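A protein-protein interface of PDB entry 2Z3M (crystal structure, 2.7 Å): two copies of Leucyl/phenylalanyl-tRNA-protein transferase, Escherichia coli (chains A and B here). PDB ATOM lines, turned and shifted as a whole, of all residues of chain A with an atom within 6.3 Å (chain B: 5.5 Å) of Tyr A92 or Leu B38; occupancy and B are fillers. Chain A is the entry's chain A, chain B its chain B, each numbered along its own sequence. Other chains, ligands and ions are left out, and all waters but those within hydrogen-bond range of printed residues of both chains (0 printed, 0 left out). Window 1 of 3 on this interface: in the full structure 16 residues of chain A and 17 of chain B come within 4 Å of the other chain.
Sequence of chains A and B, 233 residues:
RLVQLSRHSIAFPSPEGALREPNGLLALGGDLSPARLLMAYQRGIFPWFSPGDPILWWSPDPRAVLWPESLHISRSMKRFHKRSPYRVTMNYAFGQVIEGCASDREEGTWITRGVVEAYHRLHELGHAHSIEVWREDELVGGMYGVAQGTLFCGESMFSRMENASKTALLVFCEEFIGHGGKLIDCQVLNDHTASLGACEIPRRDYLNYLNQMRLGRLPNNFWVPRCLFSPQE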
ATOM      1  N   THR A  89      13.943   6.177  13.335  1.00  0.00           N
ATOM      2  CA  THR A  89      13.719   7.371  12.529  1.00  0.00           C
ATOM      3  C   THR A  89      12.307   7.912  12.716  1.00  0.00           C
ATOM      4  O   THR A  89      11.427   7.205  13.214  1.00  0.00           O
ATOM      5  CB  THR A  89      13.946   7.069  11.030  1.00  0.00           C
ATOM      6  OG1 THR A  89      13.058   6.020  10.610  1.00  0.00           O
ATOM      7  CG2 THR A  89      15.387   6.631  10.789  1.00  0.00           C
ATOM      8  N   MET A  90      12.101   9.171  12.321  1.00  0.00           N
ATOM      9  CA  MET A  90      10.788   9.810  12.429  1.00  0.00           C
ATOM     10  C   MET A  90      10.190  10.155  11.068  1.00  0.00           C
ATOM     11  O   MET A  90      10.823  10.821  10.248  1.00  0.00           O
ATOM     12  CB  MET A  90      10.874  11.087  13.262  1.00  0.00           C
ATOM     13  CG  MET A  90       9.528  11.754  13.465  1.00  0.00           C
ATOM     14  SD  MET A  90       9.653  13.221  14.484  1.00  0.00           S
ATOM     15  CE  MET A  90       9.775  12.509  16.121  1.00  0.00           C
ATOM     16  N   ASN A  91       8.964   9.697  10.839  1.00  0.00           N
ATOM     17  CA  ASN A  91       8.259   9.944   9.587  1.00  0.00           C
ATOM     18  C   ASN A  91       9.035   9.522   8.334  1.00  0.00           C
ATOM     19  O   ASN A  91       9.141  10.279   7.377  1.00  0.00           O
ATOM     20  CB  ASN A  91       7.874  11.427   9.475  1.00  0.00           C
ATOM     21  CG  ASN A  91       6.718  11.810  10.394  1.00  0.00           C
ATOM     22  OD1 ASN A  91       5.755  11.057  10.550  1.00  0.00           O
ATOM     23  ND2 ASN A  91       6.803  12.995  10.989  1.00  0.00           N
ATOM     24  N   TYR A  92       9.583   8.313   8.341  1.00  0.00           N
ATOM     25  CA  TYR A  92      10.317   7.801   7.187  1.00  0.00           C
ATOM     26  C   TYR A  92       9.375   6.942   6.354  1.00  0.00           C
ATOM     27  O   TYR A  92       9.431   6.954   5.127  1.00  0.00           O
ATOM     28  CB  TYR A  92      11.482   6.917   7.636  1.00  0.00           C
ATOM     29  CG  TYR A  92      12.861   7.519   7.497  1.00  0.00           C
ATOM     30  CD1 TYR A  92      13.174   8.744   8.090  1.00  0.00           C
ATOM     31  CD2 TYR A  92      13.875   6.825   6.835  1.00  0.00           C
ATOM     32  CE1 TYR A  92      14.461   9.261   8.035  1.00  0.00           C
ATOM     33  CE2 TYR A  92      15.164   7.332   6.775  1.00  0.00           C
ATOM     34  CZ  TYR A  92      15.450   8.551   7.379  1.00  0.00           C
ATOM     35  OH  TYR A  92      16.725   9.059   7.331  1.00  0.00           O
ATOM     36  N   ALA A  93       8.523   6.177   7.033  1.00  0.00           N
ATOM     37  CA  ALA A  93       7.586   5.296   6.356  1.00  0.00           C
ATOM     38  C   ALA A  93       6.307   5.104   7.166  1.00  0.00           C
ATOM     39  O   ALA A  93       6.044   4.019   7.686  1.00  0.00           O
ATOM     40  CB  ALA A  93       8.250   3.940   6.086  1.00  0.00           C
ATOM     41  N   PHE A  94       5.511   6.165   7.261  1.00  0.00           N
ATOM     42  CA  PHE A  94       4.254   6.122   8.003  1.00  0.00           C
ATOM     43  C   PHE A  94       3.426   4.975   7.474  1.00  0.00           C
ATOM     44  O   PHE A  94       2.971   4.137   8.235  1.00  0.00           O
ATOM     45  CB  PHE A  94       3.474   7.432   7.825  1.00  0.00           C
ATOM     46  CG  PHE A  94       2.227   7.519   8.663  1.00  0.00           C
ATOM     47  CD1 PHE A  94       2.268   8.078   9.940  1.00  0.00           C
ATOM     48  CD2 PHE A  94       1.012   7.033   8.183  1.00  0.00           C
ATOM     49  CE1 PHE A  94       1.106   8.151  10.731  1.00  0.00           C
ATOM     50  CE2 PHE A  94      -0.152   7.100   8.963  1.00  0.00           C
ATOM     51  CZ  PHE A  94      -0.103   7.659  10.238  1.00  0.00           C
ATOM     52  N   HIS A 123      -1.520  12.177   7.795  1.00  0.00           N
ATOM     53  CA  HIS A 123      -0.073  12.193   7.696  1.00  0.00           C
ATOM     54  C   HIS A 123       0.328  13.144   6.576  1.00  0.00           C
ATOM     55  O   HIS A 123       1.337  13.835   6.664  1.00  0.00           O
ATOM     56  CB  HIS A 123       0.462  10.796   7.400  1.00  0.00           C
ATOM     57  CG  HIS A 123       1.939  10.759   7.174  1.00  0.00           C
ATOM     58  ND1 HIS A 123       2.844  11.240   8.095  1.00  0.00           N
ATOM     59  CD2 HIS A 123       2.671  10.290   6.136  1.00  0.00           C
ATOM     60  CE1 HIS A 123       4.070  11.063   7.640  1.00  0.00           C
ATOM     61  NE2 HIS A 123       3.993  10.486   6.453  1.00  0.00           N
ATOM     62  N   SER A 130       4.791   9.035  12.409  1.00  0.00           N
ATOM     63  CA  SER A 130       5.257   7.695  12.718  1.00  0.00           C
ATOM     64  C   SER A 130       6.698   7.696  13.214  1.00  0.00           C
ATOM     65  O   SER A 130       7.428   8.679  13.053  1.00  0.00           O
ATOM     66  CB  SER A 130       5.121   6.776  11.487  1.00  0.00           C
ATOM     67  OG  SER A 130       5.984   7.149  10.423  1.00  0.00           O
ATOM     68  N   ILE A 131       7.081   6.583  13.831  1.00  0.00           N
ATOM     69  CA  ILE A 131       8.416   6.367  14.369  1.00  0.00           C
ATOM     70  C   ILE A 131       8.777   4.946  13.935  1.00  0.00           C
ATOM     71  O   ILE A 131       8.146   3.986  14.368  1.00  0.00           O
ATOM     72  CB  ILE A 131       8.387   6.458  15.905  1.00  0.00           C
ATOM     73  CG1 ILE A 131       7.844   7.830  16.324  1.00  0.00           C
ATOM     74  CG2 ILE A 131       9.776   6.219  16.483  1.00  0.00           C
ATOM     75  CD1 ILE A 131       6.327   7.940  16.319  1.00  0.00           C
ATOM     76  N   GLU A 132       9.781   4.814  13.074  1.00  0.00           N
ATOM     77  CA  GLU A 132      10.180   3.506  12.564  1.00  0.00           C
ATOM     78  C   GLU A 132      11.439   2.941  13.209  1.00  0.00           C
ATOM     79  O   GLU A 132      12.402   3.662  13.451  1.00  0.00           O
ATOM     80  CB  GLU A 132      10.396   3.570  11.042  1.00  0.00           C
ATOM     81  CG  GLU A 132       9.258   4.204  10.250  1.00  0.00           C
ATOM     82  CD  GLU A 132       9.344   5.722  10.207  1.00  0.00           C
ATOM     83  OE1 GLU A 132       8.324   6.377   9.913  1.00  0.00           O
ATOM     84  OE2 GLU A 132      10.438   6.264  10.456  1.00  0.00           O
ATOM     85  N   TRP A 134      14.399   0.327  12.627  1.00  0.00           N
ATOM     86  CA  TRP A 134      15.052  -0.493  11.633  1.00  0.00           C
ATOM     87  C   TRP A 134      16.161  -1.361  12.199  1.00  0.00           C
ATOM     88  O   TRP A 134      16.891  -0.961  13.107  1.00  0.00           O
ATOM     89  CB  TRP A 134      15.638   0.384  10.520  1.00  0.00           C
ATOM     90  CG  TRP A 134      14.716   1.469  10.044  1.00  0.00           C
ATOM     91  CD1 TRP A 134      14.557   2.712  10.594  1.00  0.00           C
ATOM     92  CD2 TRP A 134      13.818   1.403   8.927  1.00  0.00           C
ATOM     93  NE1 TRP A 134      13.619   3.426   9.886  1.00  0.00           N
ATOM     94  CE2 TRP A 134      13.148   2.648   8.858  1.00  0.00           C
ATOM     95  CE3 TRP A 134      13.511   0.413   7.977  1.00  0.00           C
ATOM     96  CZ2 TRP A 134      12.191   2.931   7.874  1.00  0.00           C
ATOM     97  CZ3 TRP A 134      12.559   0.691   6.999  1.00  0.00           C
ATOM     98  CH2 TRP A 134      11.910   1.943   6.957  1.00  0.00           C
ATOM     99  N   PRO A 225      11.108  14.616   8.619  1.00  0.00           N
ATOM    100  CA  PRO A 225      11.766  13.315   8.498  1.00  0.00           C
ATOM    101  C   PRO A 225      13.254  13.355   8.832  1.00  0.00           C
ATOM    102  O   PRO A 225      14.011  14.136   8.257  1.00  0.00           O
ATOM    103  CB  PRO A 225      11.501  12.941   7.044  1.00  0.00           C
ATOM    104  CG  PRO A 225      10.153  13.526   6.803  1.00  0.00           C
ATOM    105  CD  PRO A 225      10.292  14.901   7.425  1.00  0.00           C
ATOM    106  N   ARG A 226      13.662  12.513   9.774  1.00  0.00           N
ATOM    107  CA  ARG A 226      15.061  12.433  10.170  1.00  0.00           C
ATOM    108  C   ARG A 226      15.354  11.211  11.021  1.00  0.00           C
ATOM    109  O   ARG A 226      14.457  10.462  11.404  1.00  0.00           O
ATOM    110  CB  ARG A 226      15.486  13.685  10.950  1.00  0.00           C
ATOM    111  CG  ARG A 226      14.828  13.845  12.303  1.00  0.00           C
ATOM    112  CD  ARG A 226      14.010  15.119  12.313  1.00  0.00           C
ATOM    113  NE  ARG A 226      13.130  15.235  13.472  1.00  0.00           N
ATOM    114  CZ  ARG A 226      13.568  15.329  14.719  1.00  0.00           C
ATOM    115  NH1 ARG A 226      14.875  15.318  14.956  1.00  0.00           N
ATOM    116  NH2 ARG A 226      12.704  15.442  15.718  1.00  0.00           N
ATOM    117  N   CYS A 227      16.634  11.030  11.311  1.00  0.00           N
ATOM    118  CA  CYS A 227      17.102   9.930  12.129  1.00  0.00           C
ATOM    119  C   CYS A 227      17.176  10.447  13.562  1.00  0.00           C
ATOM    120  O   CYS A 227      17.703  11.532  13.806  1.00  0.00           O
ATOM    121  CB  CYS A 227      18.483   9.490  11.648  1.00  0.00           C
ATOM    122  SG  CYS A 227      19.150   8.044  12.476  1.00  0.00           S
ATOM    123  N   SER B  33      15.645   0.285  -1.250  1.00  0.00           N
ATOM    124  CA  SER B  33      14.623   0.349  -0.213  1.00  0.00           C
ATOM    125  C   SER B  33      14.419   1.800   0.231  1.00  0.00           C
ATOM    126  O   SER B  33      15.358   2.598   0.220  1.00  0.00           O
ATOM    127  CB  SER B  33      15.046  -0.510   0.985  1.00  0.00           C
ATOM    128  OG  SER B  33      16.269  -0.058   1.553  1.00  0.00           O
ATOM    129  N   PRO B  34      13.193   2.151   0.653  1.00  0.00           N
ATOM    130  CA  PRO B  34      12.835   3.509   1.105  1.00  0.00           C
ATOM    131  C   PRO B  34      13.819   4.122   2.090  1.00  0.00           C
ATOM    132  O   PRO B  34      14.364   5.197   1.858  1.00  0.00           O
ATOM    133  CB  PRO B  34      11.456   3.327   1.743  1.00  0.00           C
ATOM    134  CG  PRO B  34      10.903   2.147   1.019  1.00  0.00           C
ATOM    135  CD  PRO B  34      12.092   1.209   0.900  1.00  0.00           C
ATOM    136  N   ALA B  35      14.026   3.433   3.203  1.00  0.00           N
ATOM    137  CA  ALA B  35      14.929   3.918   4.227  1.00  0.00           C
ATOM    138  C   ALA B  35      16.345   4.209   3.701  1.00  0.00           C
ATOM    139  O   ALA B  35      16.934   5.236   4.043  1.00  0.00           O
ATOM    140  CB  ALA B  35      14.972   2.918   5.380  1.00  0.00           C
ATOM    141  N   ARG B  36      16.897   3.321   2.874  1.00  0.00           N
ATOM    142  CA  ARG B  36      18.238   3.551   2.346  1.00  0.00           C
ATOM    143  C   ARG B  36      18.270   4.765   1.429  1.00  0.00           C
ATOM    144  O   ARG B  36      19.221   5.546   1.459  1.00  0.00           O
ATOM    145  CB  ARG B  36      18.749   2.326   1.600  1.00  0.00           C
ATOM    146  CG  ARG B  36      20.113   2.526   0.956  1.00  0.00           C
ATOM    147  CD  ARG B  36      20.658   1.215   0.411  1.00  0.00           C
ATOM    148  NE  ARG B  36      21.527   0.571   1.384  1.00  0.00           N
ATOM    149  CZ  ARG B  36      21.505  -0.724   1.668  1.00  0.00           C
ATOM    150  NH1 ARG B  36      20.655  -1.527   1.054  1.00  0.00           N
ATOM    151  NH2 ARG B  36      22.325  -1.215   2.579  1.00  0.00           N
ATOM    152  N   LEU B  37      17.232   4.923   0.614  1.00  0.00           N
ATOM    153  CA  LEU B  37      17.148   6.065  -0.288  1.00  0.00           C
ATOM    154  C   LEU B  37      17.107   7.376   0.496  1.00  0.00           C
ATOM    155  O   LEU B  37      17.841   8.315   0.187  1.00  0.00           O
ATOM    156  CB  LEU B  37      15.909   5.960  -1.169  1.00  0.00           C
ATOM    157  CG  LEU B  37      16.003   4.998  -2.350  1.00  0.00           C
ATOM    158  CD1 LEU B  37      14.693   5.061  -3.129  1.00  0.00           C
ATOM    159  CD2 LEU B  37      17.186   5.376  -3.248  1.00  0.00           C
ATOM    160  N   LEU B  38      16.244   7.448   1.505  1.00  0.00           N
ATOM    161  CA  LEU B  38      16.153   8.657   2.316  1.00  0.00           C
ATOM    162  C   LEU B  38      17.503   8.915   2.955  1.00  0.00           C
ATOM    163  O   LEU B  38      18.016  10.027   2.900  1.00  0.00           O
ATOM    164  CB  LEU B  38      15.081   8.503   3.396  1.00  0.00           C
ATOM    165  CG  LEU B  38      13.735   9.185   3.141  1.00  0.00           C
ATOM    166  CD1 LEU B  38      13.465   9.336   1.642  1.00  0.00           C
ATOM    167  CD2 LEU B  38      12.647   8.358   3.810  1.00  0.00           C
ATOM    168  N   MET B  39      18.071   7.874   3.552  1.00  0.00           N
ATOM    169  CA  MET B  39      19.374   7.959   4.188  1.00  0.00           C
ATOM    170  C   MET B  39      20.344   8.649   3.219  1.00  0.00           C
ATOM    171  O   MET B  39      21.070   9.564   3.594  1.00  0.00           O
ATOM    172  CB  MET B  39      19.876   6.547   4.513  1.00  0.00           C
ATOM    173  CG  MET B  39      20.801   6.446   5.725  1.00  0.00           C
ATOM    174  SD  MET B  39      19.935   6.631   7.314  1.00  0.00           S
ATOM    175  CE  MET B  39      20.765   8.100   7.969  1.00  0.00           C
ATOM    176  N   ALA B  40      20.329   8.203   1.967  1.00  0.00           N
ATOM    177  CA  ALA B  40      21.186   8.745   0.915  1.00  0.00           C
ATOM    178  C   ALA B  40      20.926  10.213   0.597  1.00  0.00           C
ATOM    179  O   ALA B  40      21.843  11.030   0.615  1.00  0.00           O
ATOM    180  CB  ALA B  40      21.020   7.916  -0.349  1.00  0.00           C
ATOM    181  N   TYR B  41      19.679  10.545   0.282  1.00  0.00           N
ATOM    182  CA  TYR B  41      19.316  11.919  -0.055  1.00  0.00           C
ATOM    183  C   TYR B  41      19.647  12.923   1.034  1.00  0.00           C
ATOM    184  O   TYR B  41      20.032  14.064   0.747  1.00  0.00           O
ATOM    185  CB  TYR B  41      17.827  11.997  -0.397  1.00  0.00           C
ATOM    186  CG  TYR B  41      17.556  11.555  -1.805  1.00  0.00           C
ATOM    187  CD1 TYR B  41      17.714  12.435  -2.876  1.00  0.00           C
ATOM    188  CD2 TYR B  41      17.232  10.231  -2.084  1.00  0.00           C
ATOM    189  CE1 TYR B  41      17.561  12.002  -4.199  1.00  0.00           C
ATOM    190  CE2 TYR B  41      17.080   9.784  -3.402  1.00  0.00           C
ATOM    191  CZ  TYR B  41      17.248  10.673  -4.451  1.00  0.00           C
ATOM    192  OH  TYR B  41      17.119  10.217  -5.739  1.00  0.00           O
ATOM    193  N   GLN B  42      19.517  12.482   2.283  1.00  0.00           N
ATOM    194  CA  GLN B  42      19.781  13.333   3.431  1.00  0.00           C
ATOM    195  C   GLN B  42      21.262  13.572   3.657  1.00  0.00           C
ATOM    196  O   GLN B  42      21.641  14.455   4.424  1.00  0.00           O
ATOM    197  CB  GLN B  42      19.114  12.736   4.671  1.00  0.00           C
ATOM    198  CG  GLN B  42      17.598  12.596   4.473  1.00  0.00           C
ATOM    199  CD  GLN B  42      16.860  12.057   5.677  1.00  0.00           C
ATOM    200  OE1 GLN B  42      15.641  11.908   5.645  1.00  0.00           O
ATOM    201  NE2 GLN B  42      17.592  11.761   6.745  1.00  0.00           N
ATOM    202  N   ARG B  43      22.093  12.793   2.970  1.00  0.00           N
ATOM    203  CA  ARG B  43      23.544  12.927   3.063  1.00  0.00           C
ATOM    204  C   ARG B  43      24.107  13.406   1.728  1.00  0.00           C
ATOM    205  O   ARG B  43      25.310  13.303   1.478  1.00  0.00           O
ATOM    206  CB  ARG B  43      24.199  11.594   3.448  1.00  0.00           C
ATOM    207  CG  ARG B  43      24.019  11.209   4.910  1.00  0.00           C
ATOM    208  CD  ARG B  43      24.809   9.947   5.285  1.00  0.00           C
ATOM    209  NE  ARG B  43      26.261  10.111   5.157  1.00  0.00           N
ATOM    210  CZ  ARG B  43      26.986  11.002   5.831  1.00  0.00           C
ATOM    211  NH1 ARG B  43      26.401  11.824   6.692  1.00  0.00           N
ATOM    212  NH2 ARG B  43      28.298  11.065   5.653  1.00  0.00           N
ATOM    213  N   LEU B 122       8.585   5.704  -2.580  1.00  0.00           N
ATOM    214  CA  LEU B 122       8.847   6.950  -1.877  1.00  0.00           C
ATOM    215  C   LEU B 122       7.645   7.875  -2.063  1.00  0.00           C
ATOM    216  O   LEU B 122       7.284   8.638  -1.162  1.00  0.00           O
ATOM    217  CB  LEU B 122      10.086   7.637  -2.434  1.00  0.00           C
ATOM    218  CG  LEU B 122      11.455   7.052  -2.117  1.00  0.00           C
ATOM    219  CD1 LEU B 122      12.508   7.902  -2.804  1.00  0.00           C
ATOM    220  CD2 LEU B 122      11.686   7.013  -0.611  1.00  0.00           C
ATOM    221  N   LEU B 125       4.888   6.946   0.189  1.00  0.00           N
ATOM    222  CA  LEU B 125       5.233   7.274   1.562  1.00  0.00           C
ATOM    223  C   LEU B 125       5.357   8.801   1.725  1.00  0.00           C
ATOM    224  O   LEU B 125       5.770   9.307   2.783  1.00  0.00           O
ATOM    225  CB  LEU B 125       6.530   6.564   1.970  1.00  0.00           C
ATOM    226  CG  LEU B 125       6.518   5.023   2.062  1.00  0.00           C
ATOM    227  CD1 LEU B 125       7.903   4.530   2.443  1.00  0.00           C
ATOM    228  CD2 LEU B 125       5.494   4.556   3.083  1.00  0.00           C
ATOM    229  N   HIS B 127       7.411  11.184   0.092  1.00  0.00           N
ATOM    230  CA  HIS B 127       8.687  11.903  -0.014  1.00  0.00           C
ATOM    231  C   HIS B 127       9.004  12.242  -1.478  1.00  0.00           C
ATOM    232  O   HIS B 127       9.801  13.139  -1.754  1.00  0.00           O
ATOM    233  CB  HIS B 127       9.849  11.086   0.571  1.00  0.00           C
ATOM    234  CG  HIS B 127       9.677  10.724   2.014  1.00  0.00           C
ATOM    235  ND1 HIS B 127       9.355   9.449   2.430  1.00  0.00           N
ATOM    236  CD2 HIS B 127       9.777  11.470   3.140  1.00  0.00           C
ATOM    237  CE1 HIS B 127       9.266   9.426   3.748  1.00  0.00           C
ATOM    238  NE2 HIS B 127       9.517  10.639   4.203  1.00  0.00           N
ATOM    239  N   VAL B 146      12.451  14.225  -5.180  1.00  0.00           N
ATOM    240  CA  VAL B 146      12.365  14.004  -3.746  1.00  0.00           C
ATOM    241  C   VAL B 146      12.436  15.356  -3.016  1.00  0.00           C
ATOM    242  O   VAL B 146      13.241  16.216  -3.358  1.00  0.00           O
ATOM    243  CB  VAL B 146      13.529  13.070  -3.273  1.00  0.00           C
ATOM    244  CG1 VAL B 146      13.455  12.841  -1.764  1.00  0.00           C
ATOM    245  CG2 VAL B 146      13.464  11.738  -4.004  1.00  0.00           C
ATOM    246  N   GLN B 148      13.071  17.745   0.374  1.00  0.00           N
ATOM    247  CA  GLN B 148      13.925  17.777   1.552  1.00  0.00           C
ATOM    248  C   GLN B 148      13.687  19.134   2.210  1.00  0.00           C
ATOM    249  O   GLN B 148      14.554  20.001   2.199  1.00  0.00           O
ATOM    250  CB  GLN B 148      15.391  17.655   1.136  1.00  0.00           C
ATOM    251  CG  GLN B 148      16.228  16.760   2.033  1.00  0.00           C
ATOM    252  CD  GLN B 148      16.186  15.320   1.591  1.00  0.00           C
ATOM    253  OE1 GLN B 148      16.529  14.415   2.347  1.00  0.00           O
ATOM    254  NE2 GLN B 148      15.772  15.101   0.353  1.00  0.00           N
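The backbone carbonyl oxygen (O) of Asn A91 is in hydrogen-bond range of a ring nitrogen (NE2) of His B127 (3.2 Å). OH of Tyr A92 is in hydrogen-bond range of NE2 of Gln B42.
The side-chain hydroxyl (OG1) of Thr A89 is in hydrogen-bond range of the indole nitrogen (NE1) of Trp A134 (2.8 Å). The backbone NH of Asn A91 sits at hydrogen-bond distance from the backbone carbonyl oxygen of Ser A130, at 2.9 Å. OE1 of Glu A132 lies within hydrogen-bond range of N of Tyr A92, at 2.8 Å. The backbone NH (N) of Ala A93 sits at hydrogen-bond distance from the side-chain carboxylate (OE1) of Glu A132 (2.9 Å). The backbone carbonyl oxygen (O) of Leu B122 is in hydrogen-bond range of the backbone NH (N) of His B127, at 2.8 Å.
CE2 of Tyr A92 touches O of Ala B35, at 3.9 Å. CE2 of Tyr A92 touches CB of Leu B38, 3.6 Å away. Tyr A92 touches Leu B125 (O to CD1, 3.9 Å). His B127 touches Tyr A92. Ala A93 touches Leu B125 (CB to CD1, 3.7 Å). Trp A134 touches Ala B35 (CH2 to CB, 3.6 Å). O of Pro A225 touches OE1 of Gln B42 (3.8 Å). His B127 touches Pro A225.
Tyr A92 touches just these residues of chain B: Ala B35, Leu B38, Gln B42, Leu B125 and His B127. Of the printed residues of chain B, Ala A93 touches Leu B125 (3.7 Å). Of the printed residues of chain A, Leu B125 touches Tyr A92 (3.9 Å) and Ala A93 (3.7 Å). Of the printed residues of chain B, Asn A91 touches His B127 (3.2 Å). The nearest printed residue of chain A that does not touch His B127 is Ala A93 (4.7 Å).
Printed residues of chain A that touch a printed residue of chain B: Asn A91, Tyr A92, Ala A93, Trp A134 and Pro A225. Hydrophobic or aromatic side chains of chain A that line the printed part of chain B: Tyr A92, Ala A93, Trp A134 and Pro A225. Along chain A the printed residues that touch a printed residue of chain B span positions 91 to 225. Among the printed residues, 10 pairs touch across the chains. Among the printed residues, no Asp or Glu carboxylate lies within 4 Å of a Lys or Arg side-chain nitrogen of the other chain.
No position is printed for both chains. Of the 10 pairs that touch across the chains among the printed residues, none has its exchanged pair printed and touching as well.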
